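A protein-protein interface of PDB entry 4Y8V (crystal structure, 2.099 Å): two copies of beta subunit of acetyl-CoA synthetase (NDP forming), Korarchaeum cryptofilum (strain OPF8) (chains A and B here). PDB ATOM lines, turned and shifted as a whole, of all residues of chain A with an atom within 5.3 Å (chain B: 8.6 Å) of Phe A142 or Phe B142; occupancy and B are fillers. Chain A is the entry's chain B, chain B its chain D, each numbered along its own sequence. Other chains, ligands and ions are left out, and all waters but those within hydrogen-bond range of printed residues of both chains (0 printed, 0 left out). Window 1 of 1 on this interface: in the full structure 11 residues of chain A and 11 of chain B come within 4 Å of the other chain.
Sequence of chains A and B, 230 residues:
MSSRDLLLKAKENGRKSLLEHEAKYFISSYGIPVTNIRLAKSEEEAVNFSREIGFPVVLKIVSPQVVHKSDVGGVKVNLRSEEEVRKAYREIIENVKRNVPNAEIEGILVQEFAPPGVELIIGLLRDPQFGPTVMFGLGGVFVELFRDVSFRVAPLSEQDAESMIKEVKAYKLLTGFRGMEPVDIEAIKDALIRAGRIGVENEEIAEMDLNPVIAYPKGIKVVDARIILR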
ATOM      1  N   LEU A 138     -11.463 -22.878   0.370  1.00  0.00           N
ATOM      2  CA  LEU A 138     -10.433 -21.997  -0.164  1.00  0.00           C
ATOM      3  C   LEU A 138     -10.389 -20.726   0.681  1.00  0.00           C
ATOM      4  O   LEU A 138     -11.404 -20.289   1.222  1.00  0.00           O
ATOM      5  CB  LEU A 138     -10.703 -21.671  -1.634  1.00  0.00           C
ATOM      6  CG  LEU A 138     -10.174 -22.655  -2.684  1.00  0.00           C
ATOM      7  CD1 LEU A 138      -8.652 -22.632  -2.749  1.00  0.00           C
ATOM      8  CD2 LEU A 138     -10.670 -24.067  -2.418  1.00  0.00           C
ATOM      9  N   GLY A 139      -9.206 -20.136   0.798  1.00  0.00           N
ATOM     10  CA  GLY A 139      -9.012 -19.015   1.697  1.00  0.00           C
ATOM     11  C   GLY A 139      -9.641 -17.731   1.204  1.00  0.00           C
ATOM     12  O   GLY A 139     -10.257 -17.687   0.135  1.00  0.00           O
ATOM     13  N   GLY A 140      -9.472 -16.677   1.992  1.00  0.00           N
ATOM     14  CA  GLY A 140      -9.938 -15.358   1.617  1.00  0.00           C
ATOM     15  C   GLY A 140     -11.451 -15.270   1.555  1.00  0.00           C
ATOM     16  O   GLY A 140     -12.152 -15.767   2.441  1.00  0.00           O
ATOM     17  N   VAL A 141     -11.951 -14.640   0.498  1.00  0.00           N
ATOM     18  CA  VAL A 141     -13.377 -14.367   0.382  1.00  0.00           C
ATOM     19  C   VAL A 141     -14.196 -15.644   0.254  1.00  0.00           C
ATOM     20  O   VAL A 141     -15.370 -15.663   0.627  1.00  0.00           O
ATOM     21  CB  VAL A 141     -13.683 -13.464  -0.835  1.00  0.00           C
ATOM     22  CG1 VAL A 141     -13.071 -12.086  -0.641  1.00  0.00           C
ATOM     23  CG2 VAL A 141     -13.186 -14.101  -2.135  1.00  0.00           C
ATOM     24  N   PHE A 142     -13.559 -16.718  -0.201  1.00  0.00           N
ATOM     25  CA  PHE A 142     -14.294 -17.923  -0.572  1.00  0.00           C
ATOM     26  C   PHE A 142     -14.943 -18.593   0.634  1.00  0.00           C
ATOM     27  O   PHE A 142     -16.054 -19.104   0.522  1.00  0.00           O
ATOM     28  CB  PHE A 142     -13.373 -18.893  -1.309  1.00  0.00           C
ATOM     29  CG  PHE A 142     -12.913 -18.370  -2.639  1.00  0.00           C
ATOM     30  CD1 PHE A 142     -13.757 -18.408  -3.737  1.00  0.00           C
ATOM     31  CD2 PHE A 142     -11.653 -17.820  -2.787  1.00  0.00           C
ATOM     32  CE1 PHE A 142     -13.348 -17.916  -4.958  1.00  0.00           C
ATOM     33  CE2 PHE A 142     -11.238 -17.327  -4.009  1.00  0.00           C
ATOM     34  CZ  PHE A 142     -12.089 -17.374  -5.095  1.00  0.00           C
ATOM     35  N   VAL A 143     -14.270 -18.580   1.782  1.00  0.00           N
ATOM     36  CA  VAL A 143     -14.918 -19.000   3.025  1.00  0.00           C
ATOM     37  C   VAL A 143     -15.526 -17.795   3.745  1.00  0.00           C
ATOM     38  O   VAL A 143     -16.683 -17.847   4.165  1.00  0.00           O
ATOM     39  CB  VAL A 143     -13.940 -19.734   3.965  1.00  0.00           C
ATOM     40  CG1 VAL A 143     -14.543 -19.911   5.362  1.00  0.00           C
ATOM     41  CG2 VAL A 143     -13.590 -21.091   3.387  1.00  0.00           C
ATOM     42  N   GLU A 144     -14.766 -16.707   3.860  1.00  0.00           N
ATOM     43  CA  GLU A 144     -15.197 -15.559   4.660  1.00  0.00           C
ATOM     44  C   GLU A 144     -16.499 -14.940   4.163  1.00  0.00           C
ATOM     45  O   GLU A 144     -17.370 -14.591   4.959  1.00  0.00           O
ATOM     46  CB  GLU A 144     -14.124 -14.470   4.672  1.00  0.00           C
ATOM     47  CG  GLU A 144     -12.892 -14.788   5.497  1.00  0.00           C
ATOM     48  CD  GLU A 144     -12.017 -13.567   5.710  1.00  0.00           C
ATOM     49  OE1 GLU A 144     -10.811 -13.635   5.388  1.00  0.00           O
ATOM     50  OE2 GLU A 144     -12.534 -12.539   6.200  1.00  0.00           O
ATOM     51  N   LEU A 145     -16.623 -14.807   2.847  1.00  0.00           N
ATOM     52  CA  LEU A 145     -17.737 -14.082   2.243  1.00  0.00           C
ATOM     53  C   LEU A 145     -18.770 -15.012   1.612  1.00  0.00           C
ATOM     54  O   LEU A 145     -19.973 -14.834   1.814  1.00  0.00           O
ATOM     55  CB  LEU A 145     -17.203 -13.100   1.198  1.00  0.00           C
ATOM     56  CG  LEU A 145     -18.184 -12.085   0.613  1.00  0.00           C
ATOM     57  CD1 LEU A 145     -18.600 -11.051   1.652  1.00  0.00           C
ATOM     58  CD2 LEU A 145     -17.553 -11.406  -0.591  1.00  0.00           C
ATOM     59  N   PHE A 146     -18.309 -16.001   0.849  1.00  0.00           N
ATOM     60  CA  PHE A 146     -19.219 -16.892   0.129  1.00  0.00           C
ATOM     61  C   PHE A 146     -19.560 -18.163   0.911  1.00  0.00           C
ATOM     62  O   PHE A 146     -20.430 -18.924   0.494  1.00  0.00           O
ATOM     63  CB  PHE A 146     -18.618 -17.275  -1.224  1.00  0.00           C
ATOM     64  CG  PHE A 146     -18.325 -16.099  -2.112  1.00  0.00           C
ATOM     65  CD1 PHE A 146     -19.273 -15.107  -2.313  1.00  0.00           C
ATOM     66  CD2 PHE A 146     -17.102 -15.989  -2.748  1.00  0.00           C
ATOM     67  CE1 PHE A 146     -19.001 -14.026  -3.132  1.00  0.00           C
ATOM     68  CE2 PHE A 146     -16.826 -14.910  -3.568  1.00  0.00           C
ATOM     69  CZ  PHE A 146     -17.778 -13.928  -3.758  1.00  0.00           C
ATOM     70  N   ARG A 147     -18.882 -18.383   2.036  1.00  0.00           N
ATOM     71  CA  ARG A 147     -19.132 -19.555   2.881  1.00  0.00           C
ATOM     72  C   ARG A 147     -19.048 -20.870   2.096  1.00  0.00           C
ATOM     73  O   ARG A 147     -19.755 -21.831   2.380  1.00  0.00           O
ATOM     74  CB  ARG A 147     -20.502 -19.437   3.568  1.00  0.00           C
ATOM     75  CG  ARG A 147     -20.582 -18.354   4.646  1.00  0.00           C
ATOM     76  CD  ARG A 147     -19.562 -18.569   5.767  1.00  0.00           C
ATOM     77  NE  ARG A 147     -19.687 -19.880   6.404  1.00  0.00           N
ATOM     78  CZ  ARG A 147     -18.749 -20.435   7.168  1.00  0.00           C
ATOM     79  NH1 ARG A 147     -17.601 -19.804   7.389  1.00  0.00           N
ATOM     80  NH2 ARG A 147     -18.953 -21.629   7.710  1.00  0.00           N
ATOM     81  N   ASP A 148     -18.126 -20.933   1.141  1.00  0.00           N
ATOM     82  CA  ASP A 148     -17.972 -22.131   0.322  1.00  0.00           C
ATOM     83  C   ASP A 148     -17.099 -23.157   1.040  1.00  0.00           C
ATOM     84  O   ASP A 148     -15.882 -23.170   0.857  1.00  0.00           O
ATOM     85  CB  ASP A 148     -17.357 -21.777  -1.032  1.00  0.00           C
ATOM     86  CG  ASP A 148     -17.124 -22.995  -1.902  1.00  0.00           C
ATOM     87  OD1 ASP A 148     -17.944 -23.935  -1.845  1.00  0.00           O
ATOM     88  OD2 ASP A 148     -16.120 -23.012  -2.646  1.00  0.00           O
ATOM     89  N   ALA A 170     -15.032 -23.696  -5.243  1.00  0.00           N
ATOM     90  CA  ALA A 170     -13.801 -23.033  -5.679  1.00  0.00           C
ATOM     91  C   ALA A 170     -12.676 -24.046  -5.898  1.00  0.00           C
ATOM     92  O   ALA A 170     -11.493 -23.698  -5.822  1.00  0.00           O
ATOM     93  CB  ALA A 170     -13.381 -21.987  -4.664  1.00  0.00           C
ATOM     94  N   LEU A 173      -9.493 -23.750  -8.201  1.00  0.00           N
ATOM     95  CA  LEU A 173      -8.349 -22.930  -7.810  1.00  0.00           C
ATOM     96  C   LEU A 173      -7.149 -23.781  -7.397  1.00  0.00           C
ATOM     97  O   LEU A 173      -6.063 -23.254  -7.164  1.00  0.00           O
ATOM     98  CB  LEU A 173      -8.726 -21.983  -6.671  1.00  0.00           C
ATOM     99  CG  LEU A 173      -9.707 -20.867  -7.025  1.00  0.00           C
ATOM    100  CD1 LEU A 173     -10.009 -20.042  -5.793  1.00  0.00           C
ATOM    101  CD2 LEU A 173      -9.173 -19.974  -8.141  1.00  0.00           C
ATOM    102  N   VAL B 118     -12.634  -3.099  -7.907  1.00  0.00           N
ATOM    103  CA  VAL B 118     -13.240  -4.395  -8.181  1.00  0.00           C
ATOM    104  C   VAL B 118     -13.415  -4.520  -9.684  1.00  0.00           C
ATOM    105  O   VAL B 118     -14.050  -3.673 -10.300  1.00  0.00           O
ATOM    106  CB  VAL B 118     -14.595  -4.560  -7.484  1.00  0.00           C
ATOM    107  CG1 VAL B 118     -15.108  -5.986  -7.654  1.00  0.00           C
ATOM    108  CG2 VAL B 118     -14.479  -4.204  -6.009  1.00  0.00           C
ATOM    109  N   GLU B 119     -12.849  -5.565 -10.274  1.00  0.00           N
ATOM    110  CA  GLU B 119     -12.897  -5.713 -11.722  1.00  0.00           C
ATOM    111  C   GLU B 119     -14.201  -6.380 -12.145  1.00  0.00           C
ATOM    112  O   GLU B 119     -14.715  -7.257 -11.447  1.00  0.00           O
ATOM    113  CB  GLU B 119     -11.690  -6.506 -12.222  1.00  0.00           C
ATOM    114  CG  GLU B 119     -10.364  -5.888 -11.793  1.00  0.00           C
ATOM    115  CD  GLU B 119      -9.204  -6.266 -12.692  1.00  0.00           C
ATOM    116  OE1 GLU B 119      -8.149  -5.607 -12.596  1.00  0.00           O
ATOM    117  OE2 GLU B 119      -9.338  -7.219 -13.488  1.00  0.00           O
ATOM    118  N   LEU B 120     -14.732  -5.940 -13.284  1.00  0.00           N
ATOM    119  CA  LEU B 120     -15.976  -6.464 -13.835  1.00  0.00           C
ATOM    120  C   LEU B 120     -15.784  -6.812 -15.294  1.00  0.00           C
ATOM    121  O   LEU B 120     -14.860  -6.319 -15.936  1.00  0.00           O
ATOM    122  CB  LEU B 120     -17.118  -5.449 -13.731  1.00  0.00           C
ATOM    123  CG  LEU B 120     -17.299  -4.600 -12.480  1.00  0.00           C
ATOM    124  CD1 LEU B 120     -18.341  -3.526 -12.759  1.00  0.00           C
ATOM    125  CD2 LEU B 120     -17.725  -5.465 -11.317  1.00  0.00           C
ATOM    126  N   ILE B 121     -16.690  -7.634 -15.811  1.00  0.00           N
ATOM    127  CA  ILE B 121     -16.776  -7.892 -17.240  1.00  0.00           C
ATOM    128  C   ILE B 121     -18.186  -7.581 -17.717  1.00  0.00           C
ATOM    129  O   ILE B 121     -19.167  -8.061 -17.139  1.00  0.00           O
ATOM    130  CB  ILE B 121     -16.414  -9.350 -17.574  1.00  0.00           C
ATOM    131  CG1 ILE B 121     -14.956  -9.620 -17.195  1.00  0.00           C
ATOM    132  CG2 ILE B 121     -16.643  -9.639 -19.059  1.00  0.00           C
ATOM    133  CD1 ILE B 121     -14.554 -11.073 -17.276  1.00  0.00           C
ATOM    134  N   PHE B 136     -22.983 -10.138 -17.941  1.00  0.00           N
ATOM    135  CA  PHE B 136     -22.327  -9.513 -16.793  1.00  0.00           C
ATOM    136  C   PHE B 136     -21.653 -10.549 -15.915  1.00  0.00           C
ATOM    137  O   PHE B 136     -22.146 -11.669 -15.768  1.00  0.00           O
ATOM    138  CB  PHE B 136     -23.327  -8.718 -15.951  1.00  0.00           C
ATOM    139  CG  PHE B 136     -22.736  -8.169 -14.679  1.00  0.00           C
ATOM    140  CD1 PHE B 136     -21.912  -7.054 -14.704  1.00  0.00           C
ATOM    141  CD2 PHE B 136     -22.986  -8.784 -13.461  1.00  0.00           C
ATOM    142  CE1 PHE B 136     -21.361  -6.552 -13.536  1.00  0.00           C
ATOM    143  CE2 PHE B 136     -22.438  -8.287 -12.289  1.00  0.00           C
ATOM    144  CZ  PHE B 136     -21.625  -7.170 -12.328  1.00  0.00           C
ATOM    145  N   GLY B 137     -20.515 -10.171 -15.337  1.00  0.00           N
ATOM    146  CA  GLY B 137     -19.845 -11.011 -14.362  1.00  0.00           C
ATOM    147  C   GLY B 137     -18.721 -10.285 -13.649  1.00  0.00           C
ATOM    148  O   GLY B 137     -18.304  -9.206 -14.074  1.00  0.00           O
ATOM    149  N   LEU B 138     -18.236 -10.874 -12.559  1.00  0.00           N
ATOM    150  CA  LEU B 138     -17.058 -10.362 -11.865  1.00  0.00           C
ATOM    151  C   LEU B 138     -15.795 -10.774 -12.611  1.00  0.00           C
ATOM    152  O   LEU B 138     -15.752 -11.828 -13.249  1.00  0.00           O
ATOM    153  CB  LEU B 138     -17.010 -10.868 -10.421  1.00  0.00           C
ATOM    154  CG  LEU B 138     -17.775 -10.055  -9.371  1.00  0.00           C
ATOM    155  CD1 LEU B 138     -17.118  -8.697  -9.153  1.00  0.00           C
ATOM    156  CD2 LEU B 138     -19.238  -9.890  -9.754  1.00  0.00           C
ATOM    157  N   GLY B 139     -14.762  -9.942 -12.529  1.00  0.00           N
ATOM    158  CA  GLY B 139     -13.562 -10.157 -13.314  1.00  0.00           C
ATOM    159  C   GLY B 139     -12.721 -11.314 -12.814  1.00  0.00           C
ATOM    160  O   GLY B 139     -13.069 -11.979 -11.833  1.00  0.00           O
ATOM    161  N   GLY B 140     -11.603 -11.544 -13.495  1.00  0.00           N
ATOM    162  CA  GLY B 140     -10.642 -12.551 -13.087  1.00  0.00           C
ATOM    163  C   GLY B 140     -11.171 -13.966 -13.192  1.00  0.00           C
ATOM    164  O   GLY B 140     -11.796 -14.344 -14.186  1.00  0.00           O
ATOM    165  N   VAL B 141     -10.912 -14.749 -12.150  1.00  0.00           N
ATOM    166  CA  VAL B 141     -11.243 -16.164 -12.154  1.00  0.00           C
ATOM    167  C   VAL B 141     -12.750 -16.396 -12.207  1.00  0.00           C
ATOM    168  O   VAL B 141     -13.196 -17.443 -12.679  1.00  0.00           O
ATOM    169  CB  VAL B 141     -10.673 -16.880 -10.903  1.00  0.00           C
ATOM    170  CG1 VAL B 141      -9.150 -16.861 -10.923  1.00  0.00           C
ATOM    171  CG2 VAL B 141     -11.204 -16.243  -9.618  1.00  0.00           C
ATOM    172  N   PHE B 142     -13.524 -15.403 -11.779  1.00  0.00           N
ATOM    173  CA  PHE B 142     -14.958 -15.595 -11.581  1.00  0.00           C
ATOM    174  C   PHE B 142     -15.715 -15.817 -12.887  1.00  0.00           C
ATOM    175  O   PHE B 142     -16.638 -16.627 -12.929  1.00  0.00           O
ATOM    176  CB  PHE B 142     -15.536 -14.408 -10.816  1.00  0.00           C
ATOM    177  CG  PHE B 142     -15.025 -14.312  -9.411  1.00  0.00           C
ATOM    178  CD1 PHE B 142     -15.541 -15.128  -8.420  1.00  0.00           C
ATOM    179  CD2 PHE B 142     -14.004 -13.436  -9.088  1.00  0.00           C
ATOM    180  CE1 PHE B 142     -15.065 -15.060  -7.128  1.00  0.00           C
ATOM    181  CE2 PHE B 142     -13.522 -13.360  -7.797  1.00  0.00           C
ATOM    182  CZ  PHE B 142     -14.051 -14.175  -6.815  1.00  0.00           C
ATOM    183  N   VAL B 143     -15.326 -15.117 -13.948  1.00  0.00           N
ATOM    184  CA  VAL B 143     -15.848 -15.429 -15.278  1.00  0.00           C
ATOM    185  C   VAL B 143     -14.924 -16.416 -15.981  1.00  0.00           C
ATOM    186  O   VAL B 143     -15.384 -17.427 -16.512  1.00  0.00           O
ATOM    187  CB  VAL B 143     -16.017 -14.164 -16.141  1.00  0.00           C
ATOM    188  CG1 VAL B 143     -16.247 -14.521 -17.614  1.00  0.00           C
ATOM    189  CG2 VAL B 143     -17.176 -13.334 -15.622  1.00  0.00           C
ATOM    190  N   GLU B 144     -13.622 -16.147 -15.936  1.00  0.00           N
ATOM    191  CA  GLU B 144     -12.656 -16.932 -16.700  1.00  0.00           C
ATOM    192  C   GLU B 144     -12.652 -18.407 -16.287  1.00  0.00           C
ATOM    193  O   GLU B 144     -12.601 -19.293 -17.141  1.00  0.00           O
ATOM    194  CB  GLU B 144     -11.254 -16.336 -16.546  1.00  0.00           C
ATOM    195  CG  GLU B 144     -10.293 -16.692 -17.678  1.00  0.00           C
ATOM    196  CD  GLU B 144      -9.036 -15.835 -17.688  1.00  0.00           C
ATOM    197  OE1 GLU B 144      -9.001 -14.804 -16.981  1.00  0.00           O
ATOM    198  OE2 GLU B 144      -8.077 -16.192 -18.406  1.00  0.00           O
ATOM    199  N   LEU B 145     -12.725 -18.664 -14.985  1.00  0.00           N
ATOM    200  CA  LEU B 145     -12.578 -20.021 -14.452  1.00  0.00           C
ATOM    201  C   LEU B 145     -13.909 -20.635 -13.989  1.00  0.00           C
ATOM    202  O   LEU B 145     -14.204 -21.785 -14.310  1.00  0.00           O
ATOM    203  CB  LEU B 145     -11.577 -20.015 -13.294  1.00  0.00           C
ATOM    204  CG  LEU B 145     -11.100 -21.366 -12.763  1.00  0.00           C
ATOM    205  CD1 LEU B 145     -10.206 -22.066 -13.775  1.00  0.00           C
ATOM    206  CD2 LEU B 145     -10.377 -21.179 -11.439  1.00  0.00           C
ATOM    207  N   PHE B 146     -14.706 -19.869 -13.245  1.00  0.00           N
ATOM    208  CA  PHE B 146     -15.950 -20.381 -12.662  1.00  0.00           C
ATOM    209  C   PHE B 146     -17.184 -20.156 -13.542  1.00  0.00           C
ATOM    210  O   PHE B 146     -18.276 -20.608 -13.200  1.00  0.00           O
ATOM    211  CB  PHE B 146     -16.189 -19.742 -11.293  1.00  0.00           C
ATOM    212  CG  PHE B 146     -15.095 -20.005 -10.297  1.00  0.00           C
ATOM    213  CD1 PHE B 146     -14.614 -21.289 -10.092  1.00  0.00           C
ATOM    214  CD2 PHE B 146     -14.547 -18.966  -9.564  1.00  0.00           C
ATOM    215  CE1 PHE B 146     -13.609 -21.530  -9.173  1.00  0.00           C
ATOM    216  CE2 PHE B 146     -13.543 -19.200  -8.643  1.00  0.00           C
ATOM    217  CZ  PHE B 146     -13.073 -20.483  -8.448  1.00  0.00           C
ATOM    218  N   ARG B 147     -17.008 -19.428 -14.638  1.00  0.00           N
ATOM    219  CA  ARG B 147     -18.073 -19.151 -15.604  1.00  0.00           C
ATOM    220  C   ARG B 147     -19.293 -18.523 -14.915  1.00  0.00           C
ATOM    221  O   ARG B 147     -20.430 -18.740 -15.318  1.00  0.00           O
ATOM    222  CB  ARG B 147     -18.519 -20.440 -16.302  1.00  0.00           C
ATOM    223  CG  ARG B 147     -17.448 -21.196 -17.115  1.00  0.00           C
ATOM    224  CD  ARG B 147     -16.200 -20.414 -17.591  1.00  0.00           C
ATOM    225  NE  ARG B 147     -16.293 -19.277 -18.532  1.00  0.00           N
ATOM    226  CZ  ARG B 147     -17.334 -18.882 -19.270  1.00  0.00           C
ATOM    227  NH1 ARG B 147     -17.165 -17.836 -20.067  1.00  0.00           N
ATOM    228  NH2 ARG B 147     -18.525 -19.467 -19.246  1.00  0.00           N
ATOM    229  N   ASP B 148     -19.060 -17.699 -13.899  1.00  0.00           N
ATOM    230  CA  ASP B 148     -20.164 -17.106 -13.147  1.00  0.00           C
ATOM    231  C   ASP B 148     -20.692 -15.858 -13.847  1.00  0.00           C
ATOM    232  O   ASP B 148     -20.237 -14.752 -13.561  1.00  0.00           O
ATOM    233  CB  ASP B 148     -19.706 -16.763 -11.727  1.00  0.00           C
ATOM    234  CG  ASP B 148     -20.794 -16.104 -10.899  1.00  0.00           C
ATOM    235  OD1 ASP B 148     -21.976 -16.470 -11.064  1.00  0.00           O
ATOM    236  OD2 ASP B 148     -20.462 -15.221 -10.079  1.00  0.00           O
ATOM    237  N   VAL B 149     -21.670 -16.037 -14.737  1.00  0.00           N
ATOM    238  CA  VAL B 149     -22.180 -14.942 -15.568  1.00  0.00           C
ATOM    239  C   VAL B 149     -23.705 -14.905 -15.623  1.00  0.00           C
ATOM    240  O   VAL B 149     -24.361 -15.942 -15.514  1.00  0.00           O
ATOM    241  CB  VAL B 149     -21.659 -15.045 -17.016  1.00  0.00           C
ATOM    242  CG1 VAL B 149     -20.161 -14.791 -17.073  1.00  0.00           C
ATOM    243  CG2 VAL B 149     -22.002 -16.408 -17.612  1.00  0.00           C
ATOM    244  N   VAL B 168     -25.503 -12.940 -10.128  1.00  0.00           N
ATOM    245  CA  VAL B 168     -24.275 -13.726 -10.176  1.00  0.00           C
ATOM    246  C   VAL B 168     -23.843 -14.125  -8.772  1.00  0.00           C
ATOM    247  O   VAL B 168     -24.035 -13.383  -7.805  1.00  0.00           O
ATOM    248  CB  VAL B 168     -23.119 -12.977 -10.882  1.00  0.00           C
ATOM    249  CG1 VAL B 168     -23.488 -12.680 -12.334  1.00  0.00           C
ATOM    250  CG2 VAL B 168     -22.746 -11.701 -10.139  1.00  0.00           C
ATOM    251  N   LYS B 169     -23.232 -15.301  -8.689  1.00  0.00           N
ATOM    252  CA  LYS B 169     -22.858 -15.914  -7.423  1.00  0.00           C
ATOM    253  C   LYS B 169     -21.867 -15.047  -6.640  1.00  0.00           C
ATOM    254  O   LYS B 169     -21.837 -15.076  -5.408  1.00  0.00           O
ATOM    255  CB  LYS B 169     -22.240 -17.284  -7.700  1.00  0.00           C
ATOM    256  CG  LYS B 169     -23.207 -18.291  -8.319  1.00  0.00           C
ATOM    257  CD  LYS B 169     -22.443 -19.392  -9.054  1.00  0.00           C
ATOM    258  CE  LYS B 169     -23.306 -20.094 -10.097  1.00  0.00           C
ATOM    259  NZ  LYS B 169     -24.301 -21.027  -9.510  1.00  0.00           N
ATOM    260  N   ALA B 170     -21.086 -14.247  -7.359  1.00  0.00           N
ATOM    261  CA  ALA B 170     -20.039 -13.422  -6.749  1.00  0.00           C
ATOM    262  C   ALA B 170     -20.501 -11.983  -6.503  1.00  0.00           C
ATOM    263  O   ALA B 170     -19.682 -11.060  -6.450  1.00  0.00           O
ATOM    264  CB  ALA B 170     -18.798 -13.430  -7.628  1.00  0.00           C
ATOM    265  N   TYR B 171     -21.813 -11.801  -6.387  1.00  0.00           N
ATOM    266  CA  TYR B 171     -22.410 -10.476  -6.239  1.00  0.00           C
ATOM    267  C   TYR B 171     -21.893  -9.692  -5.027  1.00  0.00           C
ATOM    268  O   TYR B 171     -21.777  -8.464  -5.088  1.00  0.00           O
ATOM    269  CB  TYR B 171     -23.932 -10.601  -6.154  1.00  0.00           C
ATOM    270  CG  TYR B 171     -24.629  -9.338  -5.695  1.00  0.00           C
ATOM    271  CD1 TYR B 171     -24.600  -8.187  -6.470  1.00  0.00           C
ATOM    272  CD2 TYR B 171     -25.335  -9.305  -4.499  1.00  0.00           C
ATOM    273  CE1 TYR B 171     -25.237  -7.034  -6.060  1.00  0.00           C
ATOM    274  CE2 TYR B 171     -25.979  -8.152  -4.081  1.00  0.00           C
ATOM    275  CZ  TYR B 171     -25.926  -7.020  -4.868  1.00  0.00           C
ATOM    276  OH  TYR B 171     -26.563  -5.869  -4.467  1.00  0.00           O
ATOM    277  N   LEU B 173     -19.135  -9.322  -3.878  1.00  0.00           N
ATOM    278  CA  LEU B 173     -17.876  -8.614  -4.093  1.00  0.00           C
ATOM    279  C   LEU B 173     -18.126  -7.151  -4.451  1.00  0.00           C
ATOM    280  O   LEU B 173     -17.190  -6.358  -4.523  1.00  0.00           O
ATOM    281  CB  LEU B 173     -17.050  -9.269  -5.196  1.00  0.00           C
ATOM    282  CG  LEU B 173     -16.463 -10.652  -4.923  1.00  0.00           C
ATOM    283  CD1 LEU B 173     -15.718 -11.125  -6.155  1.00  0.00           C
ATOM    284  CD2 LEU B 173     -15.540 -10.650  -3.709  1.00  0.00           C
ATOM    285  N   PHE B 177     -16.559  -5.952   1.289  1.00  0.00           N
ATOM    286  CA  PHE B 177     -15.971  -7.091   1.984  1.00  0.00           C
ATOM    287  C   PHE B 177     -14.608  -6.693   2.538  1.00  0.00           C
ATOM    288  O   PHE B 177     -14.181  -5.551   2.368  1.00  0.00           O
ATOM    289  CB  PHE B 177     -15.848  -8.295   1.045  1.00  0.00           C
ATOM    290  CG  PHE B 177     -15.021  -8.028  -0.184  1.00  0.00           C
ATOM    291  CD1 PHE B 177     -15.576  -7.395  -1.287  1.00  0.00           C
ATOM    292  CD2 PHE B 177     -13.695  -8.427  -0.244  1.00  0.00           C
ATOM    293  CE1 PHE B 177     -14.821  -7.153  -2.422  1.00  0.00           C
ATOM    294  CE2 PHE B 177     -12.933  -8.190  -1.376  1.00  0.00           C
ATOM    295  CZ  PHE B 177     -13.496  -7.553  -2.467  1.00  0.00           C
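N of Lys B169 lies within hydrogen-bond range of OD1 of Asp B148 (2.9 Å).
OD2 of Asp A148 lies within hydrogen-bond range of N of Ala A170 (2.9 Å).
O of Phe B142 is in hydrogen-bond range of N of Arg B147 (3.3 Å).
The backbone carbonyl oxygen (O) of Phe A142 is in hydrogen-bond range of the backbone NH (N) of Arg A147 (3.3 Å).
The backbone NH (N) of Ala B170 is in hydrogen-bond range of the side-chain carboxylate (OD2) of Asp B148, at 3.0 Å.
The backbone carbonyl oxygen (O) of Val A141 is in hydrogen-bond range of the backbone NH (N) of Phe A146 (3.0 Å).
Among the printed residues, merely in contact across the chains: Val A141 with Phe B177, Phe A142 with Phe B142, Phe A142 with Phe B146, Leu A145 with Leu B173, Leu A145 with Phe B177, Phe A146 with Phe B142, Phe A146 with Lys B169, Phe A146 with Ala B170, Phe A146 with Leu B173, Ala A170 with Phe B146, Leu A173 with Leu B145 and Leu A173 with Phe B146.
Of the printed residues of chain B, Val A141 touches Phe B177 (3.7 Å).
Of chain B, only Phe B142 and Phe B146 come within 4 Å of Phe A142.
Phe B142 touches two residues of chain A.
Of the printed residues of chain A, Phe B146 touches Phe A142 (3.9 Å), Ala A170 (3.8 Å) and Leu A173 (3.7 Å).
Of the printed residues of chain A, Lys B169 touches Phe A146 (3.8 Å).
Printed residues of chain A within 4 Å of Ala B170: Phe A146.
Printed residues of chain A within 4 Å of Leu B173: Leu A145 (3.8 Å) and Phe A146 (3.7 Å).
Of the 13 printed residues of chain A, 6 touch a printed residue of chain B.
Of the 24 printed residues of chain B, 7 touch a printed residue of chain A.
Hydrophobic or aromatic side chains of chain B within 4 Å of the printed part of chain A: Phe B142, Leu B145, Phe B146, Leu B173 and Phe B177.
Along chain B the printed residues that touch a printed residue of chain A span positions 142 to 177.
Phe A142 touches Phe B146, and with the chains exchanged Phe A146 touches Phe B142.
Leu A145 touches Leu B173, and with the chains exchanged Leu A173 touches Leu B145.
Phe A146 touches Ala B170, and with the chains exchanged Ala A170 touches Phe B146.
Phe A146 touches Leu B173, and with the chains exchanged Leu A173 touches Phe B146.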
